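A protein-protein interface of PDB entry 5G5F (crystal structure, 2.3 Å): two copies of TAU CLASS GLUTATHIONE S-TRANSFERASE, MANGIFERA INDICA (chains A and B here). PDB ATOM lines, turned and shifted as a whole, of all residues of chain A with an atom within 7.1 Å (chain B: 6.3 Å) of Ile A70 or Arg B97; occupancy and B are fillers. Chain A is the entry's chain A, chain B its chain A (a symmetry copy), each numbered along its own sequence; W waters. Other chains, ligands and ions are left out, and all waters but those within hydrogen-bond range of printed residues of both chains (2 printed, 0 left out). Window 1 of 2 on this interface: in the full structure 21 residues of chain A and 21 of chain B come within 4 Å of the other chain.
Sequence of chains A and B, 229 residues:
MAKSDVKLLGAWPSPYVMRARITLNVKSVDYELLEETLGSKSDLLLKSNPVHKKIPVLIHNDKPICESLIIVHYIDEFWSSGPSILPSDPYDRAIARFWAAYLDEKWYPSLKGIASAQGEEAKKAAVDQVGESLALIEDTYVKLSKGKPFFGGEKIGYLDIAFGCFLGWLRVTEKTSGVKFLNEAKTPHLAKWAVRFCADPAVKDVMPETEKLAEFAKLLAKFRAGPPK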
ATOM      1  N   ILE A  65     -16.235  29.607 -12.296  1.00  0.00           N
ATOM      2  CA  ILE A  65     -15.601  29.109 -11.079  1.00  0.00           C
ATOM      3  C   ILE A  65     -15.358  30.293 -10.150  1.00  0.00           C
ATOM      4  O   ILE A  65     -14.638  31.226 -10.503  1.00  0.00           O
ATOM      5  CB  ILE A  65     -14.271  28.381 -11.359  1.00  0.00           C
ATOM      6  CG1 ILE A  65     -14.501  27.148 -12.236  1.00  0.00           C
ATOM      7  CG2 ILE A  65     -13.603  27.976 -10.055  1.00  0.00           C
ATOM      8  CD1 ILE A  65     -14.257  27.385 -13.710  1.00  0.00           C
ATOM      9  N   CYS A  66     -15.968  30.258  -8.970  1.00  0.00           N
ATOM     10  CA  CYS A  66     -15.918  31.394  -8.056  1.00  0.00           C
ATOM     11  C   CYS A  66     -15.018  31.138  -6.850  1.00  0.00           C
ATOM     12  O   CYS A  66     -14.613  30.000  -6.600  1.00  0.00           O
ATOM     13  CB  CYS A  66     -17.330  31.755  -7.589  1.00  0.00           C
ATOM     14  SG  CYS A  66     -18.477  32.142  -8.935  1.00  0.00           S
ATOM     15  N   GLU A  67     -14.725  32.213  -6.118  1.00  0.00           N
ATOM     16  CA  GLU A  67     -13.797  32.216  -4.982  1.00  0.00           C
ATOM     17  C   GLU A  67     -12.364  31.950  -5.434  1.00  0.00           C
ATOM     18  O   GLU A  67     -12.057  30.893  -5.987  1.00  0.00           O
ATOM     19  CB  GLU A  67     -14.224  31.203  -3.915  1.00  0.00           C
ATOM     20  CG  GLU A  67     -15.573  31.505  -3.288  1.00  0.00           C
ATOM     21  CD  GLU A  67     -15.556  32.777  -2.461  1.00  0.00           C
ATOM     22  OE1 GLU A  67     -14.539  33.030  -1.781  1.00  0.00           O
ATOM     23  OE2 GLU A  67     -16.560  33.520  -2.487  1.00  0.00           O
ATOM     24  N   SER A  68     -11.495  32.925  -5.183  1.00  0.00           N
ATOM     25  CA  SER A  68     -10.118  32.919  -5.674  1.00  0.00           C
ATOM     26  C   SER A  68      -9.324  31.675  -5.284  1.00  0.00           C
ATOM     27  O   SER A  68      -8.613  31.106  -6.110  1.00  0.00           O
ATOM     28  CB  SER A  68      -9.383  34.165  -5.175  1.00  0.00           C
ATOM     29  OG  SER A  68      -9.418  34.242  -3.761  1.00  0.00           O
ATOM     30  N   LEU A  69      -9.442  31.258  -4.028  1.00  0.00           N
ATOM     31  CA  LEU A  69      -8.698  30.101  -3.542  1.00  0.00           C
ATOM     32  C   LEU A  69      -9.206  28.808  -4.171  1.00  0.00           C
ATOM     33  O   LEU A  69      -8.444  27.862  -4.369  1.00  0.00           O
ATOM     34  CB  LEU A  69      -8.772  30.018  -2.016  1.00  0.00           C
ATOM     35  CG  LEU A  69      -7.944  31.066  -1.270  1.00  0.00           C
ATOM     36  CD1 LEU A  69      -7.986  30.820   0.228  1.00  0.00           C
ATOM     37  CD2 LEU A  69      -6.506  31.078  -1.775  1.00  0.00           C
ATOM     38  N   ILE A  70     -10.496  28.775  -4.483  1.00  0.00           N
ATOM     39  CA  ILE A  70     -11.082  27.642  -5.184  1.00  0.00           C
ATOM     40  C   ILE A  70     -10.643  27.679  -6.644  1.00  0.00           C
ATOM     41  O   ILE A  70     -10.405  26.641  -7.265  1.00  0.00           O
ATOM     42  CB  ILE A  70     -12.619  27.653  -5.080  1.00  0.00           C
ATOM     43  CG1 ILE A  70     -13.043  27.419  -3.629  1.00  0.00           C
ATOM     44  CG2 ILE A  70     -13.235  26.595  -5.981  1.00  0.00           C
ATOM     45  CD1 ILE A  70     -14.522  27.574  -3.393  1.00  0.00           C
ATOM     46  N   ILE A  71     -10.519  28.890  -7.177  1.00  0.00           N
ATOM     47  CA  ILE A  71     -10.036  29.095  -8.536  1.00  0.00           C
ATOM     48  C   ILE A  71      -8.590  28.618  -8.675  1.00  0.00           C
ATOM     49  O   ILE A  71      -8.248  27.928  -9.636  1.00  0.00           O
ATOM     50  CB  ILE A  71     -10.138  30.579  -8.948  1.00  0.00           C
ATOM     51  CG1 ILE A  71     -11.600  30.964  -9.181  1.00  0.00           C
ATOM     52  CG2 ILE A  71      -9.326  30.849 -10.205  1.00  0.00           C
ATOM     53  CD1 ILE A  71     -11.829  32.456  -9.276  1.00  0.00           C
ATOM     54  N   VAL A  72      -7.753  28.979  -7.706  1.00  0.00           N
ATOM     55  CA  VAL A  72      -6.359  28.544  -7.693  1.00  0.00           C
ATOM     56  C   VAL A  72      -6.259  27.021  -7.684  1.00  0.00           C
ATOM     57  O   VAL A  72      -5.501  26.438  -8.462  1.00  0.00           O
ATOM     58  CB  VAL A  72      -5.596  29.110  -6.478  1.00  0.00           C
ATOM     59  CG1 VAL A  72      -4.220  28.474  -6.368  1.00  0.00           C
ATOM     60  CG2 VAL A  72      -5.476  30.624  -6.583  1.00  0.00           C
ATOM     61  N   HIS A  73      -7.029  26.386  -6.803  1.00  0.00           N
ATOM     62  CA  HIS A  73      -7.107  24.927  -6.748  1.00  0.00           C
ATOM     63  C   HIS A  73      -7.499  24.345  -8.099  1.00  0.00           C
ATOM     64  O   HIS A  73      -6.890  23.387  -8.573  1.00  0.00           O
ATOM     65  CB  HIS A  73      -8.116  24.475  -5.688  1.00  0.00           C
ATOM     66  CG  HIS A  73      -7.549  24.386  -4.301  1.00  0.00           C
ATOM     67  ND1 HIS A  73      -7.329  25.507  -3.520  1.00  0.00           N
ATOM     68  CD2 HIS A  73      -7.178  23.327  -3.562  1.00  0.00           C
ATOM     69  CE1 HIS A  73      -6.836  25.123  -2.357  1.00  0.00           C
ATOM     70  NE2 HIS A  73      -6.729  23.812  -2.348  1.00  0.00           N
ATOM     71  N   TYR A  74      -8.520  24.937  -8.712  1.00  0.00           N
ATOM     72  CA  TYR A  74      -9.047  24.452  -9.982  1.00  0.00           C
ATOM     73  C   TYR A  74      -8.019  24.515 -11.103  1.00  0.00           C
ATOM     74  O   TYR A  74      -7.845  23.551 -11.849  1.00  0.00           O
ATOM     75  CB  TYR A  74     -10.291  25.247 -10.382  1.00  0.00           C
ATOM     76  CG  TYR A  74     -10.819  24.879 -11.748  1.00  0.00           C
ATOM     77  CD1 TYR A  74     -11.554  23.717 -11.938  1.00  0.00           C
ATOM     78  CD2 TYR A  74     -10.576  25.690 -12.850  1.00  0.00           C
ATOM     79  CE1 TYR A  74     -12.034  23.372 -13.186  1.00  0.00           C
ATOM     80  CE2 TYR A  74     -11.053  25.354 -14.102  1.00  0.00           C
ATOM     81  CZ  TYR A  74     -11.782  24.195 -14.263  1.00  0.00           C
ATOM     82  OH  TYR A  74     -12.260  23.856 -15.507  1.00  0.00           O
ATOM     83  N   ILE A  75      -7.350  25.657 -11.221  1.00  0.00           N
ATOM     84  CA  ILE A  75      -6.329  25.842 -12.244  1.00  0.00           C
ATOM     85  C   ILE A  75      -5.207  24.827 -12.064  1.00  0.00           C
ATOM     86  O   ILE A  75      -4.706  24.259 -13.036  1.00  0.00           O
ATOM     87  CB  ILE A  75      -5.748  27.269 -12.206  1.00  0.00           C
ATOM     88  CG1 ILE A  75      -6.848  28.299 -12.468  1.00  0.00           C
ATOM     89  CG2 ILE A  75      -4.635  27.421 -13.230  1.00  0.00           C
ATOM     90  CD1 ILE A  75      -6.410  29.730 -12.244  1.00  0.00           C
ATOM     91  N   ASP A  76      -4.831  24.588 -10.813  1.00  0.00           N
ATOM     92  CA  ASP A  76      -3.764  23.647 -10.504  1.00  0.00           C
ATOM     93  C   ASP A  76      -4.173  22.213 -10.823  1.00  0.00           C
ATOM     94  O   ASP A  76      -3.355  21.412 -11.276  1.00  0.00           O
ATOM     95  CB  ASP A  76      -3.360  23.759  -9.034  1.00  0.00           C
ATOM     96  CG  ASP A  76      -2.030  23.091  -8.744  1.00  0.00           C
ATOM     97  OD1 ASP A  76      -1.148  23.118  -9.628  1.00  0.00           O
ATOM     98  OD2 ASP A  76      -1.865  22.543  -7.634  1.00  0.00           O
ATOM     99  N   GLU A  77      -5.442  21.897 -10.590  1.00  0.00           N
ATOM    100  CA  GLU A  77      -5.934  20.537 -10.775  1.00  0.00           C
ATOM    101  C   GLU A  77      -6.303  20.236 -12.226  1.00  0.00           C
ATOM    102  O   GLU A  77      -6.173  19.099 -12.677  1.00  0.00           O
ATOM    103  CB  GLU A  77      -7.135  20.279  -9.860  1.00  0.00           C
ATOM    104  CG  GLU A  77      -6.762  20.116  -8.392  1.00  0.00           C
ATOM    105  CD  GLU A  77      -7.971  20.046  -7.480  1.00  0.00           C
ATOM    106  OE1 GLU A  77      -9.089  20.353  -7.943  1.00  0.00           O
ATOM    107  OE2 GLU A  77      -7.805  19.680  -6.297  1.00  0.00           O
ATOM    108  N   LEU A  86       0.092  23.564  -5.590  1.00  0.00           N
ATOM    109  CA  LEU A  86      -0.139  23.038  -4.249  1.00  0.00           C
ATOM    110  C   LEU A  86       0.963  22.052  -3.866  1.00  0.00           C
ATOM    111  O   LEU A  86       1.581  21.451  -4.744  1.00  0.00           O
ATOM    112  CB  LEU A  86      -1.516  22.374  -4.178  1.00  0.00           C
ATOM    113  CG  LEU A  86      -2.653  23.335  -3.829  1.00  0.00           C
ATOM    114  CD1 LEU A  86      -3.929  22.927  -4.528  1.00  0.00           C
ATOM    115  CD2 LEU A  86      -2.865  23.383  -2.324  1.00  0.00           C
ATOM    116  N   ARG A  93      -0.195  20.304   2.390  1.00  0.00           N
ATOM    117  CA  ARG A  93      -1.386  20.850   1.749  1.00  0.00           C
ATOM    118  C   ARG A  93      -2.298  21.518   2.772  1.00  0.00           C
ATOM    119  O   ARG A  93      -2.738  22.651   2.577  1.00  0.00           O
ATOM    120  CB  ARG A  93      -2.149  19.749   1.007  1.00  0.00           C
ATOM    121  CG  ARG A  93      -1.790  19.614  -0.463  1.00  0.00           C
ATOM    122  CD  ARG A  93      -2.284  18.291  -1.030  1.00  0.00           C
ATOM    123  NE  ARG A  93      -1.898  18.115  -2.427  1.00  0.00           N
ATOM    124  CZ  ARG A  93      -2.745  18.179  -3.450  1.00  0.00           C
ATOM    125  NH1 ARG A  93      -4.034  18.406  -3.235  1.00  0.00           N
ATOM    126  NH2 ARG A  93      -2.305  18.008  -4.689  1.00  0.00           N
ATOM    127  N   ARG A  97      -3.247  25.464   3.043  1.00  0.00           N
ATOM    128  CA  ARG A  97      -4.629  25.912   2.977  1.00  0.00           C
ATOM    129  C   ARG A  97      -5.055  26.679   4.225  1.00  0.00           C
ATOM    130  O   ARG A  97      -5.846  27.618   4.141  1.00  0.00           O
ATOM    131  CB  ARG A  97      -5.555  24.714   2.755  1.00  0.00           C
ATOM    132  CG  ARG A  97      -5.440  24.107   1.368  1.00  0.00           C
ATOM    133  CD  ARG A  97      -5.901  22.661   1.350  1.00  0.00           C
ATOM    134  NE  ARG A  97      -5.943  22.121  -0.005  1.00  0.00           N
ATOM    135  CZ  ARG A  97      -6.114  20.835  -0.293  1.00  0.00           C
ATOM    136  NH1 ARG A  97      -6.252  19.948   0.683  1.00  0.00           N
ATOM    137  NH2 ARG A  97      -6.141  20.435  -1.556  1.00  0.00           N
ATOM    138  N   TYR A 158       1.212  27.837  -3.556  1.00  0.00           N
ATOM    139  CA  TYR A 158      -0.108  28.231  -3.082  1.00  0.00           C
ATOM    140  C   TYR A 158      -0.070  29.394  -2.087  1.00  0.00           C
ATOM    141  O   TYR A 158      -0.772  30.388  -2.266  1.00  0.00           O
ATOM    142  CB  TYR A 158      -0.801  27.019  -2.454  1.00  0.00           C
ATOM    143  CG  TYR A 158      -2.233  27.254  -2.041  1.00  0.00           C
ATOM    144  CD1 TYR A 158      -3.241  27.352  -2.991  1.00  0.00           C
ATOM    145  CD2 TYR A 158      -2.583  27.347  -0.702  1.00  0.00           C
ATOM    146  CE1 TYR A 158      -4.554  27.558  -2.620  1.00  0.00           C
ATOM    147  CE2 TYR A 158      -3.894  27.550  -0.320  1.00  0.00           C
ATOM    148  CZ  TYR A 158      -4.877  27.656  -1.283  1.00  0.00           C
ATOM    149  OH  TYR A 158      -6.186  27.858  -0.908  1.00  0.00           O
ATOM    150  N   LEU B  69     -13.255  21.950   6.963  1.00  0.00           N
ATOM    151  CA  LEU B  69     -13.214  21.669   5.532  1.00  0.00           C
ATOM    152  C   LEU B  69     -11.804  21.311   5.075  1.00  0.00           C
ATOM    153  O   LEU B  69     -11.623  20.531   4.140  1.00  0.00           O
ATOM    154  CB  LEU B  69     -13.746  22.862   4.736  1.00  0.00           C
ATOM    155  CG  LEU B  69     -15.261  23.069   4.815  1.00  0.00           C
ATOM    156  CD1 LEU B  69     -15.699  24.196   3.896  1.00  0.00           C
ATOM    157  CD2 LEU B  69     -16.000  21.779   4.480  1.00  0.00           C
ATOM    158  N   HIS B  73     -10.608  17.559   3.649  1.00  0.00           N
ATOM    159  CA  HIS B  73      -9.659  17.423   2.545  1.00  0.00           C
ATOM    160  C   HIS B  73      -8.474  16.554   2.942  1.00  0.00           C
ATOM    161  O   HIS B  73      -8.071  15.660   2.199  1.00  0.00           O
ATOM    162  CB  HIS B  73      -9.153  18.795   2.090  1.00  0.00           C
ATOM    163  CG  HIS B  73     -10.043  19.477   1.093  1.00  0.00           C
ATOM    164  ND1 HIS B  73     -11.220  20.106   1.462  1.00  0.00           N
ATOM    165  CD2 HIS B  73      -9.925  19.639  -0.235  1.00  0.00           C
ATOM    166  CE1 HIS B  73     -11.783  20.619   0.384  1.00  0.00           C
ATOM    167  NE2 HIS B  73     -11.029  20.354  -0.661  1.00  0.00           N
ATOM    168  N   GLU B  77      -7.242  12.981   1.475  1.00  0.00           N
ATOM    169  CA  GLU B  77      -5.985  12.940   0.738  1.00  0.00           C
ATOM    170  C   GLU B  77      -4.951  12.024   1.389  1.00  0.00           C
ATOM    171  O   GLU B  77      -4.132  11.422   0.697  1.00  0.00           O
ATOM    172  CB  GLU B  77      -5.415  14.353   0.583  1.00  0.00           C
ATOM    173  CG  GLU B  77      -6.166  15.207  -0.430  1.00  0.00           C
ATOM    174  CD  GLU B  77      -5.708  16.653  -0.438  1.00  0.00           C
ATOM    175  OE1 GLU B  77      -4.977  17.055   0.491  1.00  0.00           O
ATOM    176  OE2 GLU B  77      -6.077  17.390  -1.377  1.00  0.00           O
ATOM    177  N   LEU B  86     -13.995  13.546  -2.058  1.00  0.00           N
ATOM    178  CA  LEU B  86     -14.069  14.628  -3.033  1.00  0.00           C
ATOM    179  C   LEU B  86     -14.327  14.071  -4.430  1.00  0.00           C
ATOM    180  O   LEU B  86     -13.989  12.920  -4.704  1.00  0.00           O
ATOM    181  CB  LEU B  86     -12.778  15.448  -3.001  1.00  0.00           C
ATOM    182  CG  LEU B  86     -12.784  16.582  -1.974  1.00  0.00           C
ATOM    183  CD1 LEU B  86     -11.400  16.792  -1.405  1.00  0.00           C
ATOM    184  CD2 LEU B  86     -13.300  17.866  -2.602  1.00  0.00           C
ATOM    185  N   PRO B  90     -12.080  17.926 -11.696  1.00  0.00           N
ATOM    186  CA  PRO B  90     -11.663  19.259 -11.247  1.00  0.00           C
ATOM    187  C   PRO B  90     -12.811  20.261 -11.156  1.00  0.00           C
ATOM    188  O   PRO B  90     -12.872  21.017 -10.187  1.00  0.00           O
ATOM    189  CB  PRO B  90     -10.659  19.687 -12.321  1.00  0.00           C
ATOM    190  CG  PRO B  90     -10.107  18.412 -12.836  1.00  0.00           C
ATOM    191  CD  PRO B  90     -11.252  17.442 -12.813  1.00  0.00           C
ATOM    192  N   ASP B  92     -16.102  19.505 -10.923  1.00  0.00           N
ATOM    193  CA  ASP B  92     -16.973  18.993  -9.871  1.00  0.00           C
ATOM    194  C   ASP B  92     -16.388  19.305  -8.498  1.00  0.00           C
ATOM    195  O   ASP B  92     -17.122  19.562  -7.544  1.00  0.00           O
ATOM    196  CB  ASP B  92     -17.188  17.484 -10.024  1.00  0.00           C
ATOM    197  CG  ASP B  92     -18.063  17.133 -11.212  1.00  0.00           C
ATOM    198  OD1 ASP B  92     -18.874  17.984 -11.630  1.00  0.00           O
ATOM    199  OD2 ASP B  92     -17.944  16.000 -11.722  1.00  0.00           O
ATOM    200  N   ARG B  93     -15.062  19.283  -8.410  1.00  0.00           N
ATOM    201  CA  ARG B  93     -14.360  19.632  -7.180  1.00  0.00           C
ATOM    202  C   ARG B  93     -14.609  21.089  -6.805  1.00  0.00           C
ATOM    203  O   ARG B  93     -14.955  21.396  -5.664  1.00  0.00           O
ATOM    204  CB  ARG B  93     -12.858  19.379  -7.328  1.00  0.00           C
ATOM    205  CG  ARG B  93     -12.397  18.014  -6.844  1.00  0.00           C
ATOM    206  CD  ARG B  93     -11.003  17.690  -7.360  1.00  0.00           C
ATOM    207  NE  ARG B  93     -10.564  16.357  -6.955  1.00  0.00           N
ATOM    208  CZ  ARG B  93      -9.625  16.125  -6.043  1.00  0.00           C
ATOM    209  NH1 ARG B  93      -9.014  17.138  -5.443  1.00  0.00           N
ATOM    210  NH2 ARG B  93      -9.291  14.879  -5.735  1.00  0.00           N
ATOM    211  N   ALA B  94     -14.435  21.978  -7.778  1.00  0.00           N
ATOM    212  CA  ALA B  94     -14.606  23.412  -7.567  1.00  0.00           C
ATOM    213  C   ALA B  94     -16.029  23.755  -7.142  1.00  0.00           C
ATOM    214  O   ALA B  94     -16.239  24.597  -6.268  1.00  0.00           O
ATOM    215  CB  ALA B  94     -14.238  24.176  -8.830  1.00  0.00           C
ATOM    216  N   ILE B  95     -17.001  23.099  -7.767  1.00  0.00           N
ATOM    217  CA  ILE B  95     -18.406  23.323  -7.445  1.00  0.00           C
ATOM    218  C   ILE B  95     -18.721  22.795  -6.051  1.00  0.00           C
ATOM    219  O   ILE B  95     -19.451  23.425  -5.284  1.00  0.00           O
ATOM    220  CB  ILE B  95     -19.336  22.654  -8.478  1.00  0.00           C
ATOM    221  CG1 ILE B  95     -19.084  23.229  -9.873  1.00  0.00           C
ATOM    222  CG2 ILE B  95     -20.791  22.848  -8.094  1.00  0.00           C
ATOM    223  CD1 ILE B  95     -19.031  24.742  -9.912  1.00  0.00           C
ATOM    224  N   ALA B  96     -18.161  21.632  -5.732  1.00  0.00           N
ATOM    225  CA  ALA B  96     -18.293  21.042  -4.406  1.00  0.00           C
ATOM    226  C   ALA B  96     -17.803  22.010  -3.342  1.00  0.00           C
ATOM    227  O   ALA B  96     -18.503  22.300  -2.373  1.00  0.00           O
ATOM    228  CB  ALA B  96     -17.513  19.745  -4.326  1.00  0.00           C
ATOM    229  N   ARG B  97     -16.591  22.509  -3.549  1.00  0.00           N
ATOM    230  CA  ARG B  97     -15.941  23.401  -2.602  1.00  0.00           C
ATOM    231  C   ARG B  97     -16.664  24.737  -2.467  1.00  0.00           C
ATOM    232  O   ARG B  97     -16.704  25.319  -1.383  1.00  0.00           O
ATOM    233  CB  ARG B  97     -14.486  23.630  -3.017  1.00  0.00           C
ATOM    234  CG  ARG B  97     -13.602  22.409  -2.832  1.00  0.00           C
ATOM    235  CD  ARG B  97     -12.380  22.462  -3.730  1.00  0.00           C
ATOM    236  NE  ARG B  97     -11.449  21.375  -3.444  1.00  0.00           N
ATOM    237  CZ  ARG B  97     -10.405  21.064  -4.207  1.00  0.00           C
ATOM    238  NH1 ARG B  97     -10.160  21.754  -5.311  1.00  0.00           N
ATOM    239  NH2 ARG B  97      -9.611  20.059  -3.867  1.00  0.00           N
ATOM    240  N   PHE B  98     -17.233  25.219  -3.569  1.00  0.00           N
ATOM    241  CA  PHE B  98     -17.935  26.498  -3.564  1.00  0.00           C
ATOM    242  C   PHE B  98     -19.146  26.477  -2.640  1.00  0.00           C
ATOM    243  O   PHE B  98     -19.339  27.389  -1.837  1.00  0.00           O
ATOM    244  CB  PHE B  98     -18.375  26.883  -4.978  1.00  0.00           C
ATOM    245  CG  PHE B  98     -19.325  28.047  -5.018  1.00  0.00           C
ATOM    246  CD1 PHE B  98     -18.859  29.343  -4.865  1.00  0.00           C
ATOM    247  CD2 PHE B  98     -20.684  27.847  -5.206  1.00  0.00           C
ATOM    248  CE1 PHE B  98     -19.729  30.418  -4.898  1.00  0.00           C
ATOM    249  CE2 PHE B  98     -21.559  28.919  -5.240  1.00  0.00           C
ATOM    250  CZ  PHE B  98     -21.080  30.205  -5.086  1.00  0.00           C
ATOM    251  N   TRP B  99     -19.959  25.434  -2.757  1.00  0.00           N
ATOM    252  CA  TRP B  99     -21.187  25.349  -1.978  1.00  0.00           C
ATOM    253  C   TRP B  99     -20.909  25.053  -0.511  1.00  0.00           C
ATOM    254  O   TRP B  99     -21.649  25.497   0.362  1.00  0.00           O
ATOM    255  CB  TRP B  99     -22.121  24.295  -2.573  1.00  0.00           C
ATOM    256  CG  TRP B  99     -22.750  24.761  -3.841  1.00  0.00           C
ATOM    257  CD1 TRP B  99     -22.500  24.301  -5.100  1.00  0.00           C
ATOM    258  CD2 TRP B  99     -23.713  25.812  -3.981  1.00  0.00           C
ATOM    259  NE1 TRP B  99     -23.261  24.989  -6.014  1.00  0.00           N
ATOM    260  CE2 TRP B  99     -24.013  25.923  -5.351  1.00  0.00           C
ATOM    261  CE3 TRP B  99     -24.356  26.662  -3.077  1.00  0.00           C
ATOM    262  CZ2 TRP B  99     -24.931  26.852  -5.840  1.00  0.00           C
ATOM    263  CZ3 TRP B  99     -25.265  27.583  -3.564  1.00  0.00           C
ATOM    264  CH2 TRP B  99     -25.543  27.670  -4.932  1.00  0.00           C
ATOM    265  N   ALA B 100     -19.838  24.314  -0.242  1.00  0.00           N
ATOM    266  CA  ALA B 100     -19.408  24.088   1.132  1.00  0.00           C
ATOM    267  C   ALA B 100     -19.018  25.413   1.776  1.00  0.00           C
ATOM    268  O   ALA B 100     -19.437  25.721   2.892  1.00  0.00           O
ATOM    269  CB  ALA B 100     -18.250  23.111   1.178  1.00  0.00           C
ATOM    270  N   ALA B 101     -18.217  26.196   1.058  1.00  0.00           N
ATOM    271  CA  ALA B 101     -17.805  27.515   1.524  1.00  0.00           C
ATOM    272  C   ALA B 101     -19.003  28.451   1.635  1.00  0.00           C
ATOM    273  O   ALA B 101     -19.058  29.302   2.523  1.00  0.00           O
ATOM    274  CB  ALA B 101     -16.758  28.101   0.592  1.00  0.00           C
ATOM    275  N   TYR B 102     -19.959  28.287   0.726  1.00  0.00           N
ATOM    276  CA  TYR B 102     -21.185  29.076   0.742  1.00  0.00           C
ATOM    277  C   TYR B 102     -21.996  28.820   2.006  1.00  0.00           C
ATOM    278  O   TYR B 102     -22.545  29.745   2.603  1.00  0.00           O
ATOM    279  CB  TYR B 102     -22.034  28.770  -0.493  1.00  0.00           C
ATOM    280  CG  TYR B 102     -23.467  29.240  -0.381  1.00  0.00           C
ATOM    281  CD1 TYR B 102     -23.792  30.578  -0.552  1.00  0.00           C
ATOM    282  CD2 TYR B 102     -24.496  28.347  -0.111  1.00  0.00           C
ATOM    283  CE1 TYR B 102     -25.097  31.016  -0.455  1.00  0.00           C
ATOM    284  CE2 TYR B 102     -25.806  28.775  -0.010  1.00  0.00           C
ATOM    285  CZ  TYR B 102     -26.100  30.111  -0.184  1.00  0.00           C
ATOM    286  OH  TYR B 102     -27.401  30.549  -0.087  1.00  0.00           O
ATOM    287  N   TYR B 158     -18.271  15.050  -0.294  1.00  0.00           N
ATOM    288  CA  TYR B 158     -17.852  16.304   0.316  1.00  0.00           C
ATOM    289  C   TYR B 158     -19.024  17.218   0.686  1.00  0.00           C
ATOM    290  O   TYR B 158     -19.117  17.679   1.821  1.00  0.00           O
ATOM    291  CB  TYR B 158     -16.893  17.031  -0.631  1.00  0.00           C
ATOM    292  CG  TYR B 158     -16.275  18.285  -0.066  1.00  0.00           C
ATOM    293  CD1 TYR B 158     -15.282  18.214   0.903  1.00  0.00           C
ATOM    294  CD2 TYR B 158     -16.661  19.538  -0.520  1.00  0.00           C
ATOM    295  CE1 TYR B 158     -14.706  19.357   1.418  1.00  0.00           C
ATOM    296  CE2 TYR B 158     -16.088  20.687  -0.012  1.00  0.00           C
ATOM    297  CZ  TYR B 158     -15.111  20.592   0.958  1.00  0.00           C
ATOM    298  OH  TYR B 158     -14.537  21.735   1.467  1.00  0.00           O
HETATM  299  O   HOH W   1     -11.205  23.803  -6.784  1.00  0.00           O
HETATM  300  O   HOH W   2     -10.901  22.226  -8.983  1.00  0.00           O
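The side-chain carboxylate (OE2) of Glu A77 lies within salt-bridge range of the guanidinium group (NH1) of Arg B93 (2.9 Å). The side-chain carboxylate of Glu A77 lies within salt-bridge range of the guanidinium group of Arg B97, 3.1 Å away. OE2 of Glu B77 is in salt-bridge range of NH1 of Arg A93 (2.9 Å). The guanidinium group (NH2) of Arg A97 is in salt-bridge range of the side-chain carboxylate (OE2) of Glu B77, 3.1 Å away.
ND1 of His A73 is in hydrogen-bond range of O of Leu A69 (2.7 Å). A ring nitrogen (NE2) of His A73 is in hydrogen-bond range of the guanidinium group (NE) of Arg A97 (3.0 Å). O of Leu B69 is in hydrogen-bond range of ND1 of His B73. NE of Arg B97 is in hydrogen-bond range of NE2 of His B73, 3.0 Å away.
Among the printed residues, pairs that only touch across the chains: His A73 with Arg B97 (3.4 Å), Arg A97 with His B73 (3.4 Å), Tyr A74 with Pro B90 (3.5 Å), Ile A70 with Phe B98 (3.6 Å), Ile A70 with Ala B94 (3.6 Å), Ile A70 with Arg B97 (3.7 Å), Cys A66 with Phe B98 (3.8 Å) and Glu A77 with Pro B90 (3.997 Å).
Of the printed residues of chain B, Glu A77 touches Pro B90 (3.997 Å), Arg B93 (2.9 Å) and Arg B97 (3.1 Å). Leu A86 touches none of the printed residues of chain B. Ile B95 touches none of the printed residues of chain A. No residue of chain A comes within 4 Å of Ala B96. Arg B97 touches just these residues of chain A: Ile A70 (3.7 Å), His A73 (3.4 Å) and Glu A77 (3.1 Å). Of the printed residues of chain A, Phe B98 touches Cys A66 and Ile A70. The nearest residue of chain B that does not touch Ile A70 is Ala B101 (4.6 Å). The nearest residue of chain A that does not touch Arg B97 is Arg A97 (4.2 Å). The nearest printed residue of chain A that does not touch Glu B77 is Glu A77 (5.7 Å).
Hydrophobic or aromatic side chains of chain A within 4 Å of the printed part of chain B: Ile A70, His A73 and Tyr A74. Of the 17 printed residues of chain B, 7 touch a printed residue of chain A. Hydrophobic or aromatic side chains of chain B within 4 Å of the printed part of chain A: His B73, Pro B90, Ala B94 and Phe B98. Among the printed residues, 12 pairs touch across the chains. Among the printed residues, Asp or Glu carboxylates within 4 Å of a Lys or Arg side-chain nitrogen of the other chain: Glu A77 with Arg B93 (2.9 Å), Glu A77 with Arg B97 (3.1 Å), Arg A93 with Glu B77 (2.9 Å) and Arg A97 with Glu B77 (3.1 Å).
His A73 touches Arg B97, and with the chains exchanged Arg A97 touches His B73. Glu A77 touches Arg B93, and with the chains exchanged Arg A93 touches Glu B77. Glu A77 touches Arg B97, and with the chains exchanged Arg A97 touches Glu B77. Positions printed for both chains: 69, 73, 77, 86, 93, 97 and 158. Of the 12 pairs that touch across the chains among the printed residues, 6 have their exchanged pair printed and touching as well.
Water W2 lies within hydrogen-bond range of the backbone carbonyl oxygen (O) of Pro B90 and the side-chain carboxylate (OE1) of Glu A77. Water W1 lies within hydrogen-bond range of the guanidinium group of Arg B97 (2.7 Å), the backbone carbonyl oxygen of Ile A70 (3.0 Å) and the backbone NH of Tyr A74 (3.5 Å).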
